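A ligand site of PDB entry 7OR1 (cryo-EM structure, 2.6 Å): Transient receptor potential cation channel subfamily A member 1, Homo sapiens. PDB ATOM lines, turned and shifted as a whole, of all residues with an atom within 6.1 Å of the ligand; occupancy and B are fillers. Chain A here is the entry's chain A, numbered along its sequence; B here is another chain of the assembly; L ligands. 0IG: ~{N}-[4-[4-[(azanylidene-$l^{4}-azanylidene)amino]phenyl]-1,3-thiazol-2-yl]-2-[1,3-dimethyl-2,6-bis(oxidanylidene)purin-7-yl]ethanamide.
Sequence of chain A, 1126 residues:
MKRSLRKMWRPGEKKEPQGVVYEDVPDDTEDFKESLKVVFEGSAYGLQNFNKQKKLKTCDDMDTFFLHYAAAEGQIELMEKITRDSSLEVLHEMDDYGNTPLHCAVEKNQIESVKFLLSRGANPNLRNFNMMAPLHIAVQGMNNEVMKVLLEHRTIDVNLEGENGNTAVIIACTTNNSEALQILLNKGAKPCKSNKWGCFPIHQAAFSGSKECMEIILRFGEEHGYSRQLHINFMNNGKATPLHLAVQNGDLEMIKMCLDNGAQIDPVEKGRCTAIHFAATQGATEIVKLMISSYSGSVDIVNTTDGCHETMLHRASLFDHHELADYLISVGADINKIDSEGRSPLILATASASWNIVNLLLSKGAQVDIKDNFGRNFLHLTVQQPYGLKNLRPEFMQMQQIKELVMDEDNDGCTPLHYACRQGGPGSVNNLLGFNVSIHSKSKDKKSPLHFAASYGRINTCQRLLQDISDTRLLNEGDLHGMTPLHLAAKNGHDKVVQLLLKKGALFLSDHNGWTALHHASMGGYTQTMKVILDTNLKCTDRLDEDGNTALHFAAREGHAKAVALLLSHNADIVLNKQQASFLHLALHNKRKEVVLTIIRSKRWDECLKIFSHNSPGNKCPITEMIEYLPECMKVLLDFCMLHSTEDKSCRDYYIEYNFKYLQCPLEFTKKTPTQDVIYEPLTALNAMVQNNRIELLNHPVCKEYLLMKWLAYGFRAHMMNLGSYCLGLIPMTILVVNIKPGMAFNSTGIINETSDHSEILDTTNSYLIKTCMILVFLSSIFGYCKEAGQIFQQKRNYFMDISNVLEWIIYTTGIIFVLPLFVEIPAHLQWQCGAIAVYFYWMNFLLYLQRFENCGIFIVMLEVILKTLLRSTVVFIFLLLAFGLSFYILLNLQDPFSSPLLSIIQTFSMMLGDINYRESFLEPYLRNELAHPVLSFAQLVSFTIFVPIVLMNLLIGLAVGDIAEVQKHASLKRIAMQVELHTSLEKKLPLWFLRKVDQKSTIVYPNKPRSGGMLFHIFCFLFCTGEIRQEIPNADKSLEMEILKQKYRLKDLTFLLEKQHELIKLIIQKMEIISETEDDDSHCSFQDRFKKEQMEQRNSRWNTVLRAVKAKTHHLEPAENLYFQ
Residues that only touch the ligand: Leu 707 (3.9 Å), Phe 716 (3.5 Å), Met 720 (3.6 Å), Leu 850 (3.6 Å), Arg 852 (3.97 Å), Phe 853 (3.4 Å), Gln 979 (3.5 Å) and His 983 (3.3 Å).
Hydrophobic or aromatic side chains that line the ligand: Trp 711, Phe 716, Met 720, Leu 850, Phe 853 and His 983.
Within 4 Å of the ligand: Leu 707, Trp 711, Phe 716, Met 720, Leu 850, Arg 852, Phe 853, Glu 854, Asn 855, Gln 979 and His 983.
Along chain A the residues within 4 Å of the ligand span positions 707 to 983.
The nearest printed residue that does not touch the ligand is Leu 982 (4.1 Å).
O of the ligand is in hydrogen-bond range of NE1 of Trp 711, at 3.1 Å.
OD1 of Asn 855 is in hydrogen-bond range of N4 of the ligand (3.1 Å).
N of Glu 854 lies within hydrogen-bond range of O2 of the ligand.
The backbone NH of Phe 716 is in hydrogen-bond range of the backbone carbonyl oxygen of Trp 711, at 3.2 Å.
The backbone carbonyl oxygen (O) of Gln 979 lies within hydrogen-bond range of a ring nitrogen (ND1) of His 983.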
ATOM      1  N   LEU A 707       6.748 -17.336  21.080  1.00  0.00           N
ATOM      2  CA  LEU A 707       5.734 -17.014  22.074  1.00  0.00           C
ATOM      3  C   LEU A 707       4.669 -18.096  22.154  1.00  0.00           C
ATOM      4  O   LEU A 707       4.230 -18.462  23.251  1.00  0.00           O
ATOM      5  CB  LEU A 707       5.088 -15.667  21.768  1.00  0.00           C
ATOM      6  CG  LEU A 707       5.797 -14.478  22.396  1.00  0.00           C
ATOM      7  CD1 LEU A 707       5.060 -13.210  22.081  1.00  0.00           C
ATOM      8  CD2 LEU A 707       5.905 -14.680  23.888  1.00  0.00           C
ATOM      9  N   LEU A 708       4.234 -18.620  21.010  1.00  0.00           N
ATOM     10  CA  LEU A 708       3.228 -19.683  21.030  1.00  0.00           C
ATOM     11  C   LEU A 708       3.754 -20.935  21.723  1.00  0.00           C
ATOM     12  O   LEU A 708       3.002 -21.620  22.424  1.00  0.00           O
ATOM     13  CB  LEU A 708       2.782 -19.996  19.612  1.00  0.00           C
ATOM     14  CG  LEU A 708       1.727 -21.082  19.463  1.00  0.00           C
ATOM     15  CD1 LEU A 708       0.533 -20.751  20.304  1.00  0.00           C
ATOM     16  CD2 LEU A 708       1.328 -21.213  18.019  1.00  0.00           C
ATOM     17  N   TRP A 711       3.600 -20.265  25.429  1.00  0.00           N
ATOM     18  CA  TRP A 711       2.202 -20.382  25.824  1.00  0.00           C
ATOM     19  C   TRP A 711       1.819 -21.826  26.043  1.00  0.00           C
ATOM     20  O   TRP A 711       1.617 -22.254  27.181  1.00  0.00           O
ATOM     21  CB  TRP A 711       1.316 -19.725  24.757  1.00  0.00           C
ATOM     22  CG  TRP A 711      -0.153 -19.601  25.100  1.00  0.00           C
ATOM     23  CD1 TRP A 711      -1.190 -20.060  24.344  1.00  0.00           C
ATOM     24  CD2 TRP A 711      -0.741 -18.954  26.225  1.00  0.00           C
ATOM     25  NE1 TRP A 711      -2.376 -19.750  24.945  1.00  0.00           N
ATOM     26  CE2 TRP A 711      -2.125 -19.074  26.101  1.00  0.00           C
ATOM     27  CE3 TRP A 711      -0.217 -18.291  27.343  1.00  0.00           C
ATOM     28  CZ2 TRP A 711      -3.004 -18.554  27.045  1.00  0.00           C
ATOM     29  CZ3 TRP A 711      -1.089 -17.778  28.277  1.00  0.00           C
ATOM     30  CH2 TRP A 711      -2.462 -17.914  28.122  1.00  0.00           C
ATOM     31  N   PHE A 716      -0.611 -21.221  29.302  1.00  0.00           N
ATOM     32  CA  PHE A 716      -2.025 -21.600  29.245  1.00  0.00           C
ATOM     33  C   PHE A 716      -2.425 -22.393  30.478  1.00  0.00           C
ATOM     34  O   PHE A 716      -3.476 -22.151  31.061  1.00  0.00           O
ATOM     35  CB  PHE A 716      -2.279 -22.421  27.980  1.00  0.00           C
ATOM     36  CG  PHE A 716      -3.688 -22.849  27.815  1.00  0.00           C
ATOM     37  CD1 PHE A 716      -4.612 -22.011  27.224  1.00  0.00           C
ATOM     38  CD2 PHE A 716      -4.104 -24.103  28.225  1.00  0.00           C
ATOM     39  CE1 PHE A 716      -5.913 -22.401  27.068  1.00  0.00           C
ATOM     40  CE2 PHE A 716      -5.397 -24.499  28.059  1.00  0.00           C
ATOM     41  CZ  PHE A 716      -6.306 -23.649  27.483  1.00  0.00           C
ATOM     42  N   HIS A 719      -2.486 -20.257  33.745  1.00  0.00           N
ATOM     43  CA  HIS A 719      -3.610 -19.331  33.856  1.00  0.00           C
ATOM     44  C   HIS A 719      -4.955 -20.039  33.910  1.00  0.00           C
ATOM     45  O   HIS A 719      -5.896 -19.528  34.539  1.00  0.00           O
ATOM     46  CB  HIS A 719      -3.590 -18.317  32.716  1.00  0.00           C
ATOM     47  CG  HIS A 719      -2.722 -17.137  33.000  1.00  0.00           C
ATOM     48  ND1 HIS A 719      -1.956 -17.045  34.139  1.00  0.00           N
ATOM     49  CD2 HIS A 719      -2.501 -16.003  32.306  1.00  0.00           C
ATOM     50  CE1 HIS A 719      -1.287 -15.907  34.132  1.00  0.00           C
ATOM     51  NE2 HIS A 719      -1.607 -15.252  33.020  1.00  0.00           N
ATOM     52  N   MET A 720      -5.090 -21.202  33.267  1.00  0.00           N
ATOM     53  CA  MET A 720      -6.312 -21.970  33.454  1.00  0.00           C
ATOM     54  C   MET A 720      -6.452 -22.449  34.889  1.00  0.00           C
ATOM     55  O   MET A 720      -7.562 -22.566  35.384  1.00  0.00           O
ATOM     56  CB  MET A 720      -6.351 -23.152  32.496  1.00  0.00           C
ATOM     57  CG  MET A 720      -6.733 -22.748  31.105  1.00  0.00           C
ATOM     58  SD  MET A 720      -8.348 -21.961  31.056  1.00  0.00           S
ATOM     59  CE  MET A 720      -7.990 -20.564  30.017  1.00  0.00           C
ATOM     60  N   LEU A 723      -8.025 -19.382  36.619  1.00  0.00           N
ATOM     61  CA  LEU A 723      -9.425 -19.271  36.266  1.00  0.00           C
ATOM     62  C   LEU A 723     -10.262 -20.349  36.937  1.00  0.00           C
ATOM     63  O   LEU A 723     -11.372 -20.076  37.397  1.00  0.00           O
ATOM     64  CB  LEU A 723      -9.608 -19.350  34.754  1.00  0.00           C
ATOM     65  CG  LEU A 723      -9.910 -18.035  34.065  1.00  0.00           C
ATOM     66  CD1 LEU A 723     -10.496 -18.291  32.701  1.00  0.00           C
ATOM     67  CD2 LEU A 723     -10.851 -17.214  34.901  1.00  0.00           C
ATOM     68  N   PHE A 846     -14.580 -10.661  37.671  1.00  0.00           N
ATOM     69  CA  PHE A 846     -14.217 -11.623  36.626  1.00  0.00           C
ATOM     70  C   PHE A 846     -13.556 -10.954  35.413  1.00  0.00           C
ATOM     71  O   PHE A 846     -12.766 -11.603  34.696  1.00  0.00           O
ATOM     72  CB  PHE A 846     -15.460 -12.391  36.191  1.00  0.00           C
ATOM     73  CG  PHE A 846     -15.175 -13.626  35.423  1.00  0.00           C
ATOM     74  CD1 PHE A 846     -14.418 -14.643  35.972  1.00  0.00           C
ATOM     75  CD2 PHE A 846     -15.694 -13.804  34.163  1.00  0.00           C
ATOM     76  CE1 PHE A 846     -14.164 -15.783  35.266  1.00  0.00           C
ATOM     77  CE2 PHE A 846     -15.442 -14.952  33.451  1.00  0.00           C
ATOM     78  CZ  PHE A 846     -14.676 -15.937  34.006  1.00  0.00           C
ATOM     79  N   LEU A 850     -10.332 -11.886  32.932  1.00  0.00           N
ATOM     80  CA  LEU A 850     -10.391 -11.969  31.471  1.00  0.00           C
ATOM     81  C   LEU A 850      -9.365 -11.078  30.786  1.00  0.00           C
ATOM     82  O   LEU A 850      -9.020 -11.329  29.630  1.00  0.00           O
ATOM     83  CB  LEU A 850     -11.763 -11.581  30.956  1.00  0.00           C
ATOM     84  CG  LEU A 850     -12.861 -12.636  31.020  1.00  0.00           C
ATOM     85  CD1 LEU A 850     -13.968 -12.204  30.099  1.00  0.00           C
ATOM     86  CD2 LEU A 850     -12.334 -13.983  30.635  1.00  0.00           C
ATOM     87  N   ARG A 852      -6.380 -10.892  30.706  1.00  0.00           N
ATOM     88  CA  ARG A 852      -5.081 -11.467  30.365  1.00  0.00           C
ATOM     89  C   ARG A 852      -5.049 -11.951  28.919  1.00  0.00           C
ATOM     90  O   ARG A 852      -4.080 -11.710  28.199  1.00  0.00           O
ATOM     91  CB  ARG A 852      -4.741 -12.612  31.299  1.00  0.00           C
ATOM     92  CG  ARG A 852      -4.955 -12.290  32.751  1.00  0.00           C
ATOM     93  CD  ARG A 852      -3.720 -11.681  33.386  1.00  0.00           C
ATOM     94  NE  ARG A 852      -4.035 -11.101  34.678  1.00  0.00           N
ATOM     95  CZ  ARG A 852      -4.314 -11.812  35.767  1.00  0.00           C
ATOM     96  NH1 ARG A 852      -4.310 -13.131  35.754  1.00  0.00           N
ATOM     97  NH2 ARG A 852      -4.609 -11.175  36.898  1.00  0.00           N
ATOM     98  N   PHE A 853      -6.101 -12.633  28.497  1.00  0.00           N
ATOM     99  CA  PHE A 853      -6.141 -13.235  27.169  1.00  0.00           C
ATOM    100  C   PHE A 853      -6.111 -12.159  26.098  1.00  0.00           C
ATOM    101  O   PHE A 853      -6.559 -11.034  26.310  1.00  0.00           O
ATOM    102  CB  PHE A 853      -7.369 -14.109  27.030  1.00  0.00           C
ATOM    103  CG  PHE A 853      -7.510 -15.103  28.130  1.00  0.00           C
ATOM    104  CD1 PHE A 853      -6.781 -16.268  28.114  1.00  0.00           C
ATOM    105  CD2 PHE A 853      -8.347 -14.866  29.194  1.00  0.00           C
ATOM    106  CE1 PHE A 853      -6.893 -17.186  29.131  1.00  0.00           C
ATOM    107  CE2 PHE A 853      -8.461 -15.770  30.209  1.00  0.00           C
ATOM    108  CZ  PHE A 853      -7.736 -16.930  30.186  1.00  0.00           C
ATOM    109  N   GLU A 854      -5.552 -12.502  24.944  1.00  0.00           N
ATOM    110  CA  GLU A 854      -5.181 -11.472  23.977  1.00  0.00           C
ATOM    111  C   GLU A 854      -6.346 -11.087  23.081  1.00  0.00           C
ATOM    112  O   GLU A 854      -6.442  -9.929  22.652  1.00  0.00           O
ATOM    113  CB  GLU A 854      -3.995 -11.942  23.145  1.00  0.00           C
ATOM    114  CG  GLU A 854      -4.260 -13.163  22.311  1.00  0.00           C
ATOM    115  CD  GLU A 854      -4.234 -12.867  20.829  1.00  0.00           C
ATOM    116  OE1 GLU A 854      -4.117 -11.677  20.469  1.00  0.00           O
ATOM    117  OE2 GLU A 854      -4.339 -13.817  20.029  1.00  0.00           O
ATOM    118  N   ASN A 855      -7.235 -12.025  22.786  1.00  0.00           N
ATOM    119  CA  ASN A 855      -8.344 -11.700  21.895  1.00  0.00           C
ATOM    120  C   ASN A 855      -9.350 -10.766  22.525  1.00  0.00           C
ATOM    121  O   ASN A 855     -10.143 -10.149  21.802  1.00  0.00           O
ATOM    122  CB  ASN A 855      -9.032 -12.980  21.434  1.00  0.00           C
ATOM    123  CG  ASN A 855      -9.205 -13.985  22.556  1.00  0.00           C
ATOM    124  OD1 ASN A 855      -8.257 -14.652  22.962  1.00  0.00           O
ATOM    125  ND2 ASN A 855     -10.422 -14.094  23.063  1.00  0.00           N
ATOM    126  N   CYS A 856      -9.338 -10.622  23.852  1.00  0.00           N
ATOM    127  CA  CYS A 856     -10.341  -9.825  24.539  1.00  0.00           C
ATOM    128  C   CYS A 856      -9.793  -9.007  25.692  1.00  0.00           C
ATOM    129  O   CYS A 856     -10.514  -8.751  26.650  1.00  0.00           O
ATOM    130  CB  CYS A 856     -11.456 -10.740  25.064  1.00  0.00           C
ATOM    131  SG  CYS A 856     -10.948 -11.928  26.312  1.00  0.00           S
ATOM    132  N   GLN A 979       1.695 -10.085  26.596  1.00  0.00           N
ATOM    133  CA  GLN A 979       2.072 -11.495  26.621  1.00  0.00           C
ATOM    134  C   GLN A 979       3.513 -11.665  27.070  1.00  0.00           C
ATOM    135  O   GLN A 979       3.826 -12.581  27.850  1.00  0.00           O
ATOM    136  CB  GLN A 979       1.889 -12.103  25.243  1.00  0.00           C
ATOM    137  CG  GLN A 979       0.544 -11.831  24.624  1.00  0.00           C
ATOM    138  CD  GLN A 979       0.477 -12.284  23.190  1.00  0.00           C
ATOM    139  OE1 GLN A 979       1.465 -12.754  22.634  1.00  0.00           O
ATOM    140  NE2 GLN A 979      -0.680 -12.139  22.575  1.00  0.00           N
ATOM    141  N   LEU A 982       3.592 -11.222  30.775  1.00  0.00           N
ATOM    142  CA  LEU A 982       2.982 -12.389  31.402  1.00  0.00           C
ATOM    143  C   LEU A 982       3.992 -13.517  31.559  1.00  0.00           C
ATOM    144  O   LEU A 982       4.232 -14.014  32.671  1.00  0.00           O
ATOM    145  CB  LEU A 982       1.789 -12.854  30.564  1.00  0.00           C
ATOM    146  CG  LEU A 982       0.719 -13.808  31.102  1.00  0.00           C
ATOM    147  CD1 LEU A 982      -0.431 -13.812  30.149  1.00  0.00           C
ATOM    148  CD2 LEU A 982       1.244 -15.221  31.261  1.00  0.00           C
ATOM    149  N   HIS A 983       4.613 -13.922  30.448  1.00  0.00           N
ATOM    150  CA  HIS A 983       5.535 -15.048  30.532  1.00  0.00           C
ATOM    151  C   HIS A 983       6.797 -14.708  31.306  1.00  0.00           C
ATOM    152  O   HIS A 983       7.336 -15.561  32.019  1.00  0.00           O
ATOM    153  CB  HIS A 983       5.889 -15.538  29.135  1.00  0.00           C
ATOM    154  CG  HIS A 983       4.739 -16.174  28.432  1.00  0.00           C
ATOM    155  ND1 HIS A 983       3.962 -15.513  27.514  1.00  0.00           N
ATOM    156  CD2 HIS A 983       4.218 -17.422  28.534  1.00  0.00           C
ATOM    157  CE1 HIS A 983       3.020 -16.328  27.067  1.00  0.00           C
ATOM    158  NE2 HIS A 983       3.149 -17.486  27.670  1.00  0.00           N
ATOM    159  N   VAL B 875     -18.301 -11.158  23.933  1.00  0.00           N
ATOM    160  CA  VAL B 875     -17.626 -12.126  24.786  1.00  0.00           C
ATOM    161  C   VAL B 875     -17.142 -11.501  26.076  1.00  0.00           C
ATOM    162  O   VAL B 875     -16.849 -12.217  27.032  1.00  0.00           O
ATOM    163  CB  VAL B 875     -16.456 -12.787  24.024  1.00  0.00           C
ATOM    164  CG1 VAL B 875     -16.901 -13.211  22.645  1.00  0.00           C
ATOM    165  CG2 VAL B 875     -15.290 -11.830  23.929  1.00  0.00           C
ATOM    166  N   PHE B 879     -20.919  -9.946  30.552  1.00  0.00           N
ATOM    167  CA  PHE B 879     -20.829 -10.202  31.985  1.00  0.00           C
ATOM    168  C   PHE B 879     -21.236  -8.980  32.799  1.00  0.00           C
ATOM    169  O   PHE B 879     -21.666  -9.135  33.942  1.00  0.00           O
ATOM    170  CB  PHE B 879     -19.420 -10.654  32.336  1.00  0.00           C
ATOM    171  CG  PHE B 879     -19.023 -11.920  31.660  1.00  0.00           C
ATOM    172  CD1 PHE B 879     -19.733 -13.087  31.861  1.00  0.00           C
ATOM    173  CD2 PHE B 879     -17.933 -11.953  30.815  1.00  0.00           C
ATOM    174  CE1 PHE B 879     -19.375 -14.245  31.234  1.00  0.00           C
ATOM    175  CE2 PHE B 879     -17.573 -13.125  30.189  1.00  0.00           C
ATOM    176  CZ  PHE B 879     -18.294 -14.272  30.399  1.00  0.00           C
HETATM  177  O   0IG L   1      -5.070 -18.712  23.698  1.00  0.00           O
HETATM  178  C   0IG L   1      -5.654 -17.701  23.337  1.00  0.00           C
HETATM  179  N   0IG L   1      -3.631 -16.842  22.272  1.00  0.00           N
HETATM  180  C5  0IG L   1      -2.074 -14.665  26.463  1.00  0.00           C
HETATM  181  C4  0IG L   1      -0.616 -15.591  24.760  1.00  0.00           C
HETATM  182  C3  0IG L   1      -1.548 -16.610  22.818  1.00  0.00           C
HETATM  183  C2  0IG L   1      -2.820 -17.362  21.325  1.00  0.00           C
HETATM  184  C1  0IG L   1      -5.093 -16.813  22.251  1.00  0.00           C
HETATM  185  N1  0IG L   1      -1.547 -17.245  21.620  1.00  0.00           N
HETATM  186  C10 0IG L   1      -9.100 -18.135  26.405  1.00  0.00           C
HETATM  187  C11 0IG L   1     -10.358 -17.725  27.053  1.00  0.00           C
HETATM  188  C12 0IG L   1     -11.126 -16.692  26.536  1.00  0.00           C
HETATM  189  C13 0IG L   1     -12.307 -16.306  27.149  1.00  0.00           C
HETATM  190  C14 0IG L   1     -12.749 -16.966  28.286  1.00  0.00           C
HETATM  191  C15 0IG L   1     -11.991 -18.001  28.807  1.00  0.00           C
HETATM  192  C16 0IG L   1     -10.808 -18.378  28.199  1.00  0.00           C
HETATM  193  C17 0IG L   1      -8.328 -19.196  26.747  1.00  0.00           C
HETATM  194  C6  0IG L   1       0.899 -16.497  23.068  1.00  0.00           C
HETATM  195  C7  0IG L   1      -2.809 -16.350  23.257  1.00  0.00           C
HETATM  196  C8  0IG L   1      -3.081 -15.703  24.494  1.00  0.00           C
HETATM  197  C9  0IG L   1      -7.498 -17.890  24.919  1.00  0.00           C
HETATM  198  N2  0IG L   1      -0.451 -16.244  23.552  1.00  0.00           N
HETATM  199  N3  0IG L   1      -1.916 -15.350  25.180  1.00  0.00           N
HETATM  200  N4  0IG L   1      -6.834 -17.282  23.865  1.00  0.00           N
HETATM  201  N5  0IG L   1      -8.618 -17.384  25.341  1.00  0.00           N
HETATM  202  N6  0IG L   1     -13.972 -16.636  28.936  1.00  0.00           N
HETATM  203  N7  0IG L   1     -14.523 -17.530  29.669  1.00  0.00           N
HETATM  204  N8  0IG L   1     -15.012 -18.331  30.325  1.00  0.00           N
HETATM  205  O1  0IG L   1       0.335 -15.257  25.429  1.00  0.00           O
HETATM  206  O2  0IG L   1      -4.179 -15.443  24.951  1.00  0.00           O
HETATM  207  S   0IG L   1      -6.942 -19.309  25.743  1.00  0.00           S
